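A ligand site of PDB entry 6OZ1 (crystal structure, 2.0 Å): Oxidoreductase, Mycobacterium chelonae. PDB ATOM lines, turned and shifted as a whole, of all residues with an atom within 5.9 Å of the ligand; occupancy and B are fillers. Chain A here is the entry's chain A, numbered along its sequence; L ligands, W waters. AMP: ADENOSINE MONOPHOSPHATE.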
ATOM      1  N   THR A 263     -13.300  13.473  28.717  1.00  0.00           N
ATOM      2  CA  THR A 263     -12.551  13.045  27.567  1.00  0.00           C
ATOM      3  C   THR A 263     -12.008  14.282  26.869  1.00  0.00           C
ATOM      4  O   THR A 263     -12.597  15.368  26.960  1.00  0.00           O
ATOM      5  CB  THR A 263     -13.438  12.243  26.623  1.00  0.00           C
ATOM      6  OG1 THR A 263     -12.625  11.654  25.596  1.00  0.00           O
ATOM      7  CG2 THR A 263     -14.493  13.147  26.004  1.00  0.00           C
ATOM      8  N   HIS A 306     -12.256   6.096  33.529  1.00  0.00           N
ATOM      9  CA  HIS A 306     -12.352   5.664  32.128  1.00  0.00           C
ATOM     10  C   HIS A 306     -13.452   4.611  31.974  1.00  0.00           C
ATOM     11  O   HIS A 306     -13.639   3.761  32.853  1.00  0.00           O
ATOM     12  CB  HIS A 306     -11.014   5.113  31.606  1.00  0.00           C
ATOM     13  CG  HIS A 306     -10.974   4.920  30.119  1.00  0.00           C
ATOM     14  ND1 HIS A 306     -11.519   3.822  29.507  1.00  0.00           N
ATOM     15  CD2 HIS A 306     -10.473   5.699  29.131  1.00  0.00           C
ATOM     16  CE1 HIS A 306     -11.353   3.922  28.199  1.00  0.00           C
ATOM     17  NE2 HIS A 306     -10.711   5.054  27.942  1.00  0.00           N
ATOM     18  N   LEU A 307     -14.198   4.703  30.871  1.00  0.00           N
ATOM     19  CA  LEU A 307     -15.292   3.780  30.636  1.00  0.00           C
ATOM     20  C   LEU A 307     -14.837   2.337  30.782  1.00  0.00           C
ATOM     21  O   LEU A 307     -15.542   1.506  31.376  1.00  0.00           O
ATOM     22  CB  LEU A 307     -15.903   4.022  29.253  1.00  0.00           C
ATOM     23  CG  LEU A 307     -17.104   3.132  28.880  1.00  0.00           C
ATOM     24  CD1 LEU A 307     -18.174   3.199  29.977  1.00  0.00           C
ATOM     25  CD2 LEU A 307     -17.730   3.560  27.538  1.00  0.00           C
ATOM     26  N   SER A 399     -10.189  -7.101  23.557  1.00  0.00           N
ATOM     27  CA  SER A 399      -9.465  -5.857  23.683  1.00  0.00           C
ATOM     28  C   SER A 399     -10.308  -4.744  23.104  1.00  0.00           C
ATOM     29  O   SER A 399     -11.156  -4.999  22.232  1.00  0.00           O
ATOM     30  CB  SER A 399      -8.113  -5.944  22.969  1.00  0.00           C
ATOM     31  OG  SER A 399      -7.296  -4.858  23.329  1.00  0.00           O
ATOM     32  N   GLY A 400     -10.060  -3.515  23.553  1.00  0.00           N
ATOM     33  CA  GLY A 400     -10.727  -2.349  23.017  1.00  0.00           C
ATOM     34  C   GLY A 400     -10.079  -1.085  23.552  1.00  0.00           C
ATOM     35  O   GLY A 400      -9.100  -1.131  24.296  1.00  0.00           O
ATOM     36  N   SER A 401     -10.657   0.059  23.162  1.00  0.00           N
ATOM     37  CA  SER A 401     -10.281   1.430  23.506  1.00  0.00           C
ATOM     38  C   SER A 401      -9.227   1.969  22.556  1.00  0.00           C
ATOM     39  O   SER A 401      -8.991   3.173  22.527  1.00  0.00           O
ATOM     40  CB  SER A 401      -9.768   1.600  24.950  1.00  0.00           C
ATOM     41  OG  SER A 401      -8.426   1.137  25.034  1.00  0.00           O
ATOM     42  N   ALA A 402      -8.585   1.104  21.770  1.00  0.00           N
ATOM     43  CA  ALA A 402      -7.555   1.502  20.819  1.00  0.00           C
ATOM     44  C   ALA A 402      -7.320   0.303  19.864  1.00  0.00           C
ATOM     45  O   ALA A 402      -7.725  -0.834  20.174  1.00  0.00           O
ATOM     46  CB  ALA A 402      -6.256   1.905  21.542  1.00  0.00           C
ATOM     47  N   PRO A 403      -6.722   0.543  18.692  1.00  0.00           N
ATOM     48  CA  PRO A 403      -6.491  -0.565  17.750  1.00  0.00           C
ATOM     49  C   PRO A 403      -5.473  -1.572  18.262  1.00  0.00           C
ATOM     50  O   PRO A 403      -4.548  -1.223  19.007  1.00  0.00           O
ATOM     51  CB  PRO A 403      -5.962   0.144  16.496  1.00  0.00           C
ATOM     52  CG  PRO A 403      -5.420   1.460  16.991  1.00  0.00           C
ATOM     53  CD  PRO A 403      -6.361   1.848  18.118  1.00  0.00           C
ATOM     54  N   LEU A 404      -5.623  -2.823  17.813  1.00  0.00           N
ATOM     55  CA  LEU A 404      -4.749  -3.943  18.159  1.00  0.00           C
ATOM     56  C   LEU A 404      -4.300  -4.627  16.871  1.00  0.00           C
ATOM     57  O   LEU A 404      -5.125  -4.940  16.022  1.00  0.00           O
ATOM     58  CB  LEU A 404      -5.469  -4.948  19.081  1.00  0.00           C
ATOM     59  CG  LEU A 404      -4.623  -6.028  19.755  1.00  0.00           C
ATOM     60  CD1 LEU A 404      -3.680  -5.425  20.808  1.00  0.00           C
ATOM     61  CD2 LEU A 404      -5.505  -7.181  20.354  1.00  0.00           C
ATOM     62  N   ASP A 422     -12.698  -8.210  19.461  1.00  0.00           N
ATOM     63  CA  ASP A 422     -12.378  -6.801  19.284  1.00  0.00           C
ATOM     64  C   ASP A 422     -13.640  -5.988  19.564  1.00  0.00           C
ATOM     65  O   ASP A 422     -14.650  -6.140  18.865  1.00  0.00           O
ATOM     66  CB  ASP A 422     -11.843  -6.522  17.882  1.00  0.00           C
ATOM     67  CG  ASP A 422     -11.793  -5.023  17.576  1.00  0.00           C
ATOM     68  OD1 ASP A 422     -11.322  -4.230  18.438  1.00  0.00           O
ATOM     69  OD2 ASP A 422     -12.252  -4.631  16.482  1.00  0.00           O
ATOM     70  N   GLY A 423     -13.584  -5.152  20.609  1.00  0.00           N
ATOM     71  CA  GLY A 423     -14.716  -4.335  20.981  1.00  0.00           C
ATOM     72  C   GLY A 423     -14.460  -2.876  20.666  1.00  0.00           C
ATOM     73  O   GLY A 423     -13.600  -2.250  21.283  1.00  0.00           O
ATOM     74  N   TYR A 424     -15.195  -2.314  19.703  1.00  0.00           N
ATOM     75  CA  TYR A 424     -15.047  -0.896  19.392  1.00  0.00           C
ATOM     76  C   TYR A 424     -16.236  -0.143  19.949  1.00  0.00           C
ATOM     77  O   TYR A 424     -17.372  -0.619  19.885  1.00  0.00           O
ATOM     78  CB  TYR A 424     -14.894  -0.653  17.880  1.00  0.00           C
ATOM     79  CG  TYR A 424     -15.131   0.816  17.482  1.00  0.00           C
ATOM     80  CD1 TYR A 424     -14.116   1.771  17.553  1.00  0.00           C
ATOM     81  CD2 TYR A 424     -16.398   1.235  17.043  1.00  0.00           C
ATOM     82  CE1 TYR A 424     -14.341   3.130  17.165  1.00  0.00           C
ATOM     83  CE2 TYR A 424     -16.641   2.547  16.658  1.00  0.00           C
ATOM     84  CZ  TYR A 424     -15.628   3.488  16.733  1.00  0.00           C
ATOM     85  OH  TYR A 424     -15.902   4.777  16.391  1.00  0.00           O
ATOM     86  N   GLY A 425     -15.947   1.010  20.565  1.00  0.00           N
ATOM     87  CA  GLY A 425     -16.963   1.876  21.132  1.00  0.00           C
ATOM     88  C   GLY A 425     -16.317   3.152  21.615  1.00  0.00           C
ATOM     89  O   GLY A 425     -15.134   3.379  21.414  1.00  0.00           O
ATOM     90  N   SER A 426     -17.118   3.986  22.265  1.00  0.00           N
ATOM     91  CA  SER A 426     -16.615   5.246  22.781  1.00  0.00           C
ATOM     92  C   SER A 426     -17.393   5.639  24.027  1.00  0.00           C
ATOM     93  O   SER A 426     -18.476   5.126  24.303  1.00  0.00           O
ATOM     94  CB  SER A 426     -16.706   6.348  21.701  1.00  0.00           C
ATOM     95  OG  SER A 426     -18.065   6.468  21.261  1.00  0.00           O
ATOM     96  N   THR A 427     -16.788   6.533  24.806  1.00  0.00           N
ATOM     97  CA  THR A 427     -17.516   7.172  25.894  1.00  0.00           C
ATOM     98  C   THR A 427     -18.850   7.752  25.406  1.00  0.00           C
ATOM     99  O   THR A 427     -19.881   7.605  26.067  1.00  0.00           O
ATOM    100  CB  THR A 427     -16.637   8.256  26.521  1.00  0.00           C
ATOM    101  OG1 THR A 427     -15.391   7.675  26.933  1.00  0.00           O
ATOM    102  CG2 THR A 427     -17.343   8.913  27.720  1.00  0.00           C
ATOM    103  N   GLU A 428     -18.838   8.381  24.224  1.00  0.00           N
ATOM    104  CA  GLU A 428     -20.028   9.049  23.705  1.00  0.00           C
ATOM    105  C   GLU A 428     -21.081   8.050  23.262  1.00  0.00           C
ATOM    106  O   GLU A 428     -22.236   8.117  23.690  1.00  0.00           O
ATOM    107  CB  GLU A 428     -19.649   9.961  22.548  1.00  0.00           C
ATOM    108  CG  GLU A 428     -18.878  11.215  22.984  1.00  0.00           C
ATOM    109  CD  GLU A 428     -17.379  10.986  23.125  1.00  0.00           C
ATOM    110  OE1 GLU A 428     -16.684  11.987  23.289  1.00  0.00           O
ATOM    111  OE2 GLU A 428     -16.911   9.841  23.051  1.00  0.00           O
ATOM    112  N   TRP A 433     -19.195  -1.981  18.003  1.00  0.00           N
ATOM    113  CA  TRP A 433     -19.055  -3.241  17.256  1.00  0.00           C
ATOM    114  C   TRP A 433     -18.273  -4.311  18.008  1.00  0.00           C
ATOM    115  O   TRP A 433     -17.529  -4.041  18.946  1.00  0.00           O
ATOM    116  CB  TRP A 433     -18.423  -3.050  15.859  1.00  0.00           C
ATOM    117  CG  TRP A 433     -16.884  -2.837  15.685  1.00  0.00           C
ATOM    118  CD1 TRP A 433     -15.844  -3.606  16.203  1.00  0.00           C
ATOM    119  CD2 TRP A 433     -16.262  -1.843  14.848  1.00  0.00           C
ATOM    120  NE1 TRP A 433     -14.629  -3.123  15.730  1.00  0.00           N
ATOM    121  CE2 TRP A 433     -14.858  -2.052  14.902  1.00  0.00           C
ATOM    122  CE3 TRP A 433     -16.752  -0.779  14.079  1.00  0.00           C
ATOM    123  CZ2 TRP A 433     -13.968  -1.241  14.240  1.00  0.00           C
ATOM    124  CZ3 TRP A 433     -15.849   0.044  13.414  1.00  0.00           C
ATOM    125  CH2 TRP A 433     -14.480  -0.193  13.484  1.00  0.00           C
ATOM    126  N   THR A 498     -18.003  10.227  14.804  1.00  0.00           N
ATOM    127  CA  THR A 498     -17.063   9.537  15.688  1.00  0.00           C
ATOM    128  C   THR A 498     -15.655  10.113  15.624  1.00  0.00           C
ATOM    129  O   THR A 498     -14.872   9.903  16.563  1.00  0.00           O
ATOM    130  CB  THR A 498     -16.930   8.044  15.352  1.00  0.00           C
ATOM    131  OG1 THR A 498     -16.408   7.922  14.015  1.00  0.00           O
ATOM    132  CG2 THR A 498     -18.239   7.282  15.510  1.00  0.00           C
ATOM    133  N   GLY A 499     -15.283  10.783  14.532  1.00  0.00           N
ATOM    134  CA  GLY A 499     -13.887  11.171  14.351  1.00  0.00           C
ATOM    135  C   GLY A 499     -12.962  10.005  14.049  1.00  0.00           C
ATOM    136  O   GLY A 499     -11.729  10.155  14.124  1.00  0.00           O
ATOM    137  N   ASP A 500     -13.534   8.854  13.702  1.00  0.00           N
ATOM    138  CA  ASP A 500     -12.793   7.651  13.355  1.00  0.00           C
ATOM    139  C   ASP A 500     -12.980   7.326  11.866  1.00  0.00           C
ATOM    140  O   ASP A 500     -14.103   7.304  11.374  1.00  0.00           O
ATOM    141  CB  ASP A 500     -13.285   6.469  14.190  1.00  0.00           C
ATOM    142  CG  ASP A 500     -12.909   6.595  15.671  1.00  0.00           C
ATOM    143  OD1 ASP A 500     -11.826   7.146  15.930  1.00  0.00           O
ATOM    144  OD2 ASP A 500     -13.675   6.158  16.556  1.00  0.00           O
ATOM    145  N   TYR A 512     -11.438  -0.726  11.461  1.00  0.00           N
ATOM    146  CA  TYR A 512     -10.893   0.541  11.971  1.00  0.00           C
ATOM    147  C   TYR A 512      -9.609   0.901  11.222  1.00  0.00           C
ATOM    148  O   TYR A 512      -8.718   0.062  11.069  1.00  0.00           O
ATOM    149  CB  TYR A 512     -10.609   0.421  13.463  1.00  0.00           C
ATOM    150  CG  TYR A 512     -10.119   1.702  14.150  1.00  0.00           C
ATOM    151  CD1 TYR A 512     -11.007   2.612  14.703  1.00  0.00           C
ATOM    152  CD2 TYR A 512      -8.751   1.943  14.316  1.00  0.00           C
ATOM    153  CE1 TYR A 512     -10.546   3.785  15.376  1.00  0.00           C
ATOM    154  CE2 TYR A 512      -8.281   3.104  15.005  1.00  0.00           C
ATOM    155  CZ  TYR A 512      -9.203   4.011  15.518  1.00  0.00           C
ATOM    156  OH  TYR A 512      -8.762   5.134  16.181  1.00  0.00           O
ATOM    157  N   ARG A 515      -7.927   7.372  13.815  1.00  0.00           N
ATOM    158  CA  ARG A 515      -8.563   8.659  14.041  1.00  0.00           C
ATOM    159  C   ARG A 515      -8.332   9.563  12.837  1.00  0.00           C
ATOM    160  O   ARG A 515      -7.213   9.633  12.296  1.00  0.00           O
ATOM    161  CB  ARG A 515      -7.975   9.351  15.298  1.00  0.00           C
ATOM    162  CG  ARG A 515      -8.057   8.558  16.596  1.00  0.00           C
ATOM    163  CD  ARG A 515      -9.423   8.598  17.240  1.00  0.00           C
ATOM    164  NE  ARG A 515      -9.867   9.957  17.534  1.00  0.00           N
ATOM    165  CZ  ARG A 515     -11.150  10.313  17.657  1.00  0.00           C
ATOM    166  NH1 ARG A 515     -12.109   9.421  17.510  1.00  0.00           N
ATOM    167  NH2 ARG A 515     -11.462  11.569  17.911  1.00  0.00           N
ATOM    168  N   LYS A 623      -3.294   5.162  26.033  1.00  0.00           N
ATOM    169  CA  LYS A 623      -3.067   5.589  24.660  1.00  0.00           C
ATOM    170  C   LYS A 623      -2.127   6.792  24.668  1.00  0.00           C
ATOM    171  O   LYS A 623      -2.078   7.562  25.632  1.00  0.00           O
ATOM    172  CB  LYS A 623      -4.391   5.970  23.975  1.00  0.00           C
ATOM    173  CG  LYS A 623      -5.338   4.801  23.688  1.00  0.00           C
ATOM    174  CD  LYS A 623      -6.674   5.276  23.031  1.00  0.00           C
ATOM    175  CE  LYS A 623      -7.705   5.644  24.093  1.00  0.00           C
ATOM    176  NZ  LYS A 623      -9.105   5.867  23.552  1.00  0.00           N
HETATM  177  P   AMP L   1     -12.707   7.316  24.508  1.00  0.00           P
HETATM  178  O1P AMP L   1     -12.902   6.077  25.362  1.00  0.00           O
HETATM  179  O2P AMP L   1     -13.951   8.089  24.106  1.00  0.00           O
HETATM  180  O3P AMP L   1     -11.709   8.239  25.187  1.00  0.00           O
HETATM  181  O5' AMP L   1     -12.034   6.776  23.170  1.00  0.00           O
HETATM  182  C5' AMP L   1     -12.820   6.262  22.099  1.00  0.00           C
HETATM  183  C4' AMP L   1     -11.967   6.070  20.860  1.00  0.00           C
HETATM  184  O4' AMP L   1     -11.026   4.988  21.076  1.00  0.00           O
HETATM  185  C3' AMP L   1     -12.689   5.667  19.589  1.00  0.00           C
HETATM  186  O3' AMP L   1     -13.332   6.734  18.937  1.00  0.00           O
HETATM  187  C2' AMP L   1     -11.557   5.066  18.759  1.00  0.00           C
HETATM  188  O2' AMP L   1     -10.748   6.073  18.180  1.00  0.00           O
HETATM  189  C1' AMP L   1     -10.744   4.369  19.839  1.00  0.00           C
HETATM  190  N9  AMP L   1     -11.052   2.921  19.869  1.00  0.00           N
HETATM  191  C8  AMP L   1     -11.887   2.616  20.890  1.00  0.00           C
HETATM  192  N7  AMP L   1     -12.112   1.288  20.810  1.00  0.00           N
HETATM  193  C5  AMP L   1     -11.417   0.804  19.742  1.00  0.00           C
HETATM  194  C6  AMP L   1     -11.250  -0.434  19.168  1.00  0.00           C
HETATM  195  N6  AMP L   1     -11.761  -1.763  19.453  1.00  0.00           N
HETATM  196  N1  AMP L   1     -10.507  -0.577  18.092  1.00  0.00           N
HETATM  197  C2  AMP L   1      -9.865   0.459  17.527  1.00  0.00           C
HETATM  198  N3  AMP L   1     -10.007   1.682  18.078  1.00  0.00           N
HETATM  199  C4  AMP L   1     -10.787   1.834  19.172  1.00  0.00           C
HETATM  200  O   HOH W   1     -14.259   9.262  21.080  1.00  0.00           O
HETATM  201  O   HOH W   2     -10.675  -2.330  15.979  1.00  0.00           O
HETATM  202  O   HOH W   3     -15.856   8.852  18.838  1.00  0.00           O
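An oxygen (O3') of the ligand is in hydrogen-bond range of the side-chain carboxylate (OD2) of Asp 500 (2.5 Å).
A nitrogen (N6) of the ligand lies within hydrogen-bond range of the backbone carbonyl oxygen (O) of Gly 423.
N6 of the ligand lies within hydrogen-bond range of OD1 of Asp 422.
The side-chain hydroxyl (OH) of Tyr 512 lies within hydrogen-bond range of an oxygen (O2') of the ligand, 3.0 Å away.
The guanidinium group of Arg 515 lies within hydrogen-bond range of an oxygen (O3') of the ligand, 3.3 Å away.
The backbone NH of Ser 401 lies within hydrogen-bond range of a nitrogen (N7) of the ligand (3.0 Å).
The side-chain amino group (NZ) of Lys 623 is in salt-bridge range of an oxygen (O3P) of the ligand (3.9 Å).
The backbone NH of Thr 427 is in hydrogen-bond range of an oxygen (O2P) of the ligand (3.3 Å).
An oxygen (O2P) of the ligand is in hydrogen-bond range of the side-chain hydroxyl of Thr 427, 3.2 Å away.
The side-chain carboxylate (OD1) of Asp 500 lies within salt-bridge range of the guanidinium group (NH1) of Arg 515, at 2.8 Å.
The side-chain hydroxyl of Tyr 424 lies within hydrogen-bond range of the side-chain carboxylate of Asp 500 (2.6 Å).
The backbone NH of Asp 500 sits at hydrogen-bond distance from the side-chain hydroxyl of Thr 498, at 3.0 Å.
The backbone NH (N) of Gly 423 lies within hydrogen-bond range of the backbone carbonyl oxygen (O) of Ser 399.
OD2 of Asp 422 lies within hydrogen-bond range of NE1 of Trp 433 (2.9 Å).
The backbone NH (N) of Arg 515 sits at hydrogen-bond distance from the side-chain hydroxyl (OH) of Tyr 512, 3.4 Å away.
The backbone carbonyl oxygen (O) of Thr 498 is in hydrogen-bond range of the guanidinium group (NH1) of Arg 515, 3.0 Å away.
N of Trp 433 is in hydrogen-bond range of O of Tyr 424, 3.0 Å away.
Water W2 lies within hydrogen-bond range of a nitrogen (N1) of the ligand (2.8 Å) and the side-chain carboxylate (OD2) of Asp 422 (2.8 Å).
Water W1 bridges O2P of the ligand (3.3 Å) and OE2 of Glu 428 (3.4 Å).
Water W3 bridges O of Thr 498 (2.7 Å) and O3' of the ligand (3.3 Å).
N1 of the ligand sits close to O of Ala 402 (3.5 Å).
N of Tyr 424 sits close to N6 of the ligand (3.5 Å).
OG1 of Thr 263 touches O3P of the ligand (3.6 Å).
His 306 touches the ligand (NE2 to O1P, 3.5 Å).
Gly 400 touches the ligand.
N of Pro 403 touches C2 of the ligand, 3.4 Å away.
Gly 425 touches the ligand.
Ser 426 touches the ligand.
OE2 of Glu 428 touches O2P of the ligand, at 3.6 Å.
The nearest printed residue that does not touch the ligand is Thr 498 (4.2 Å).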
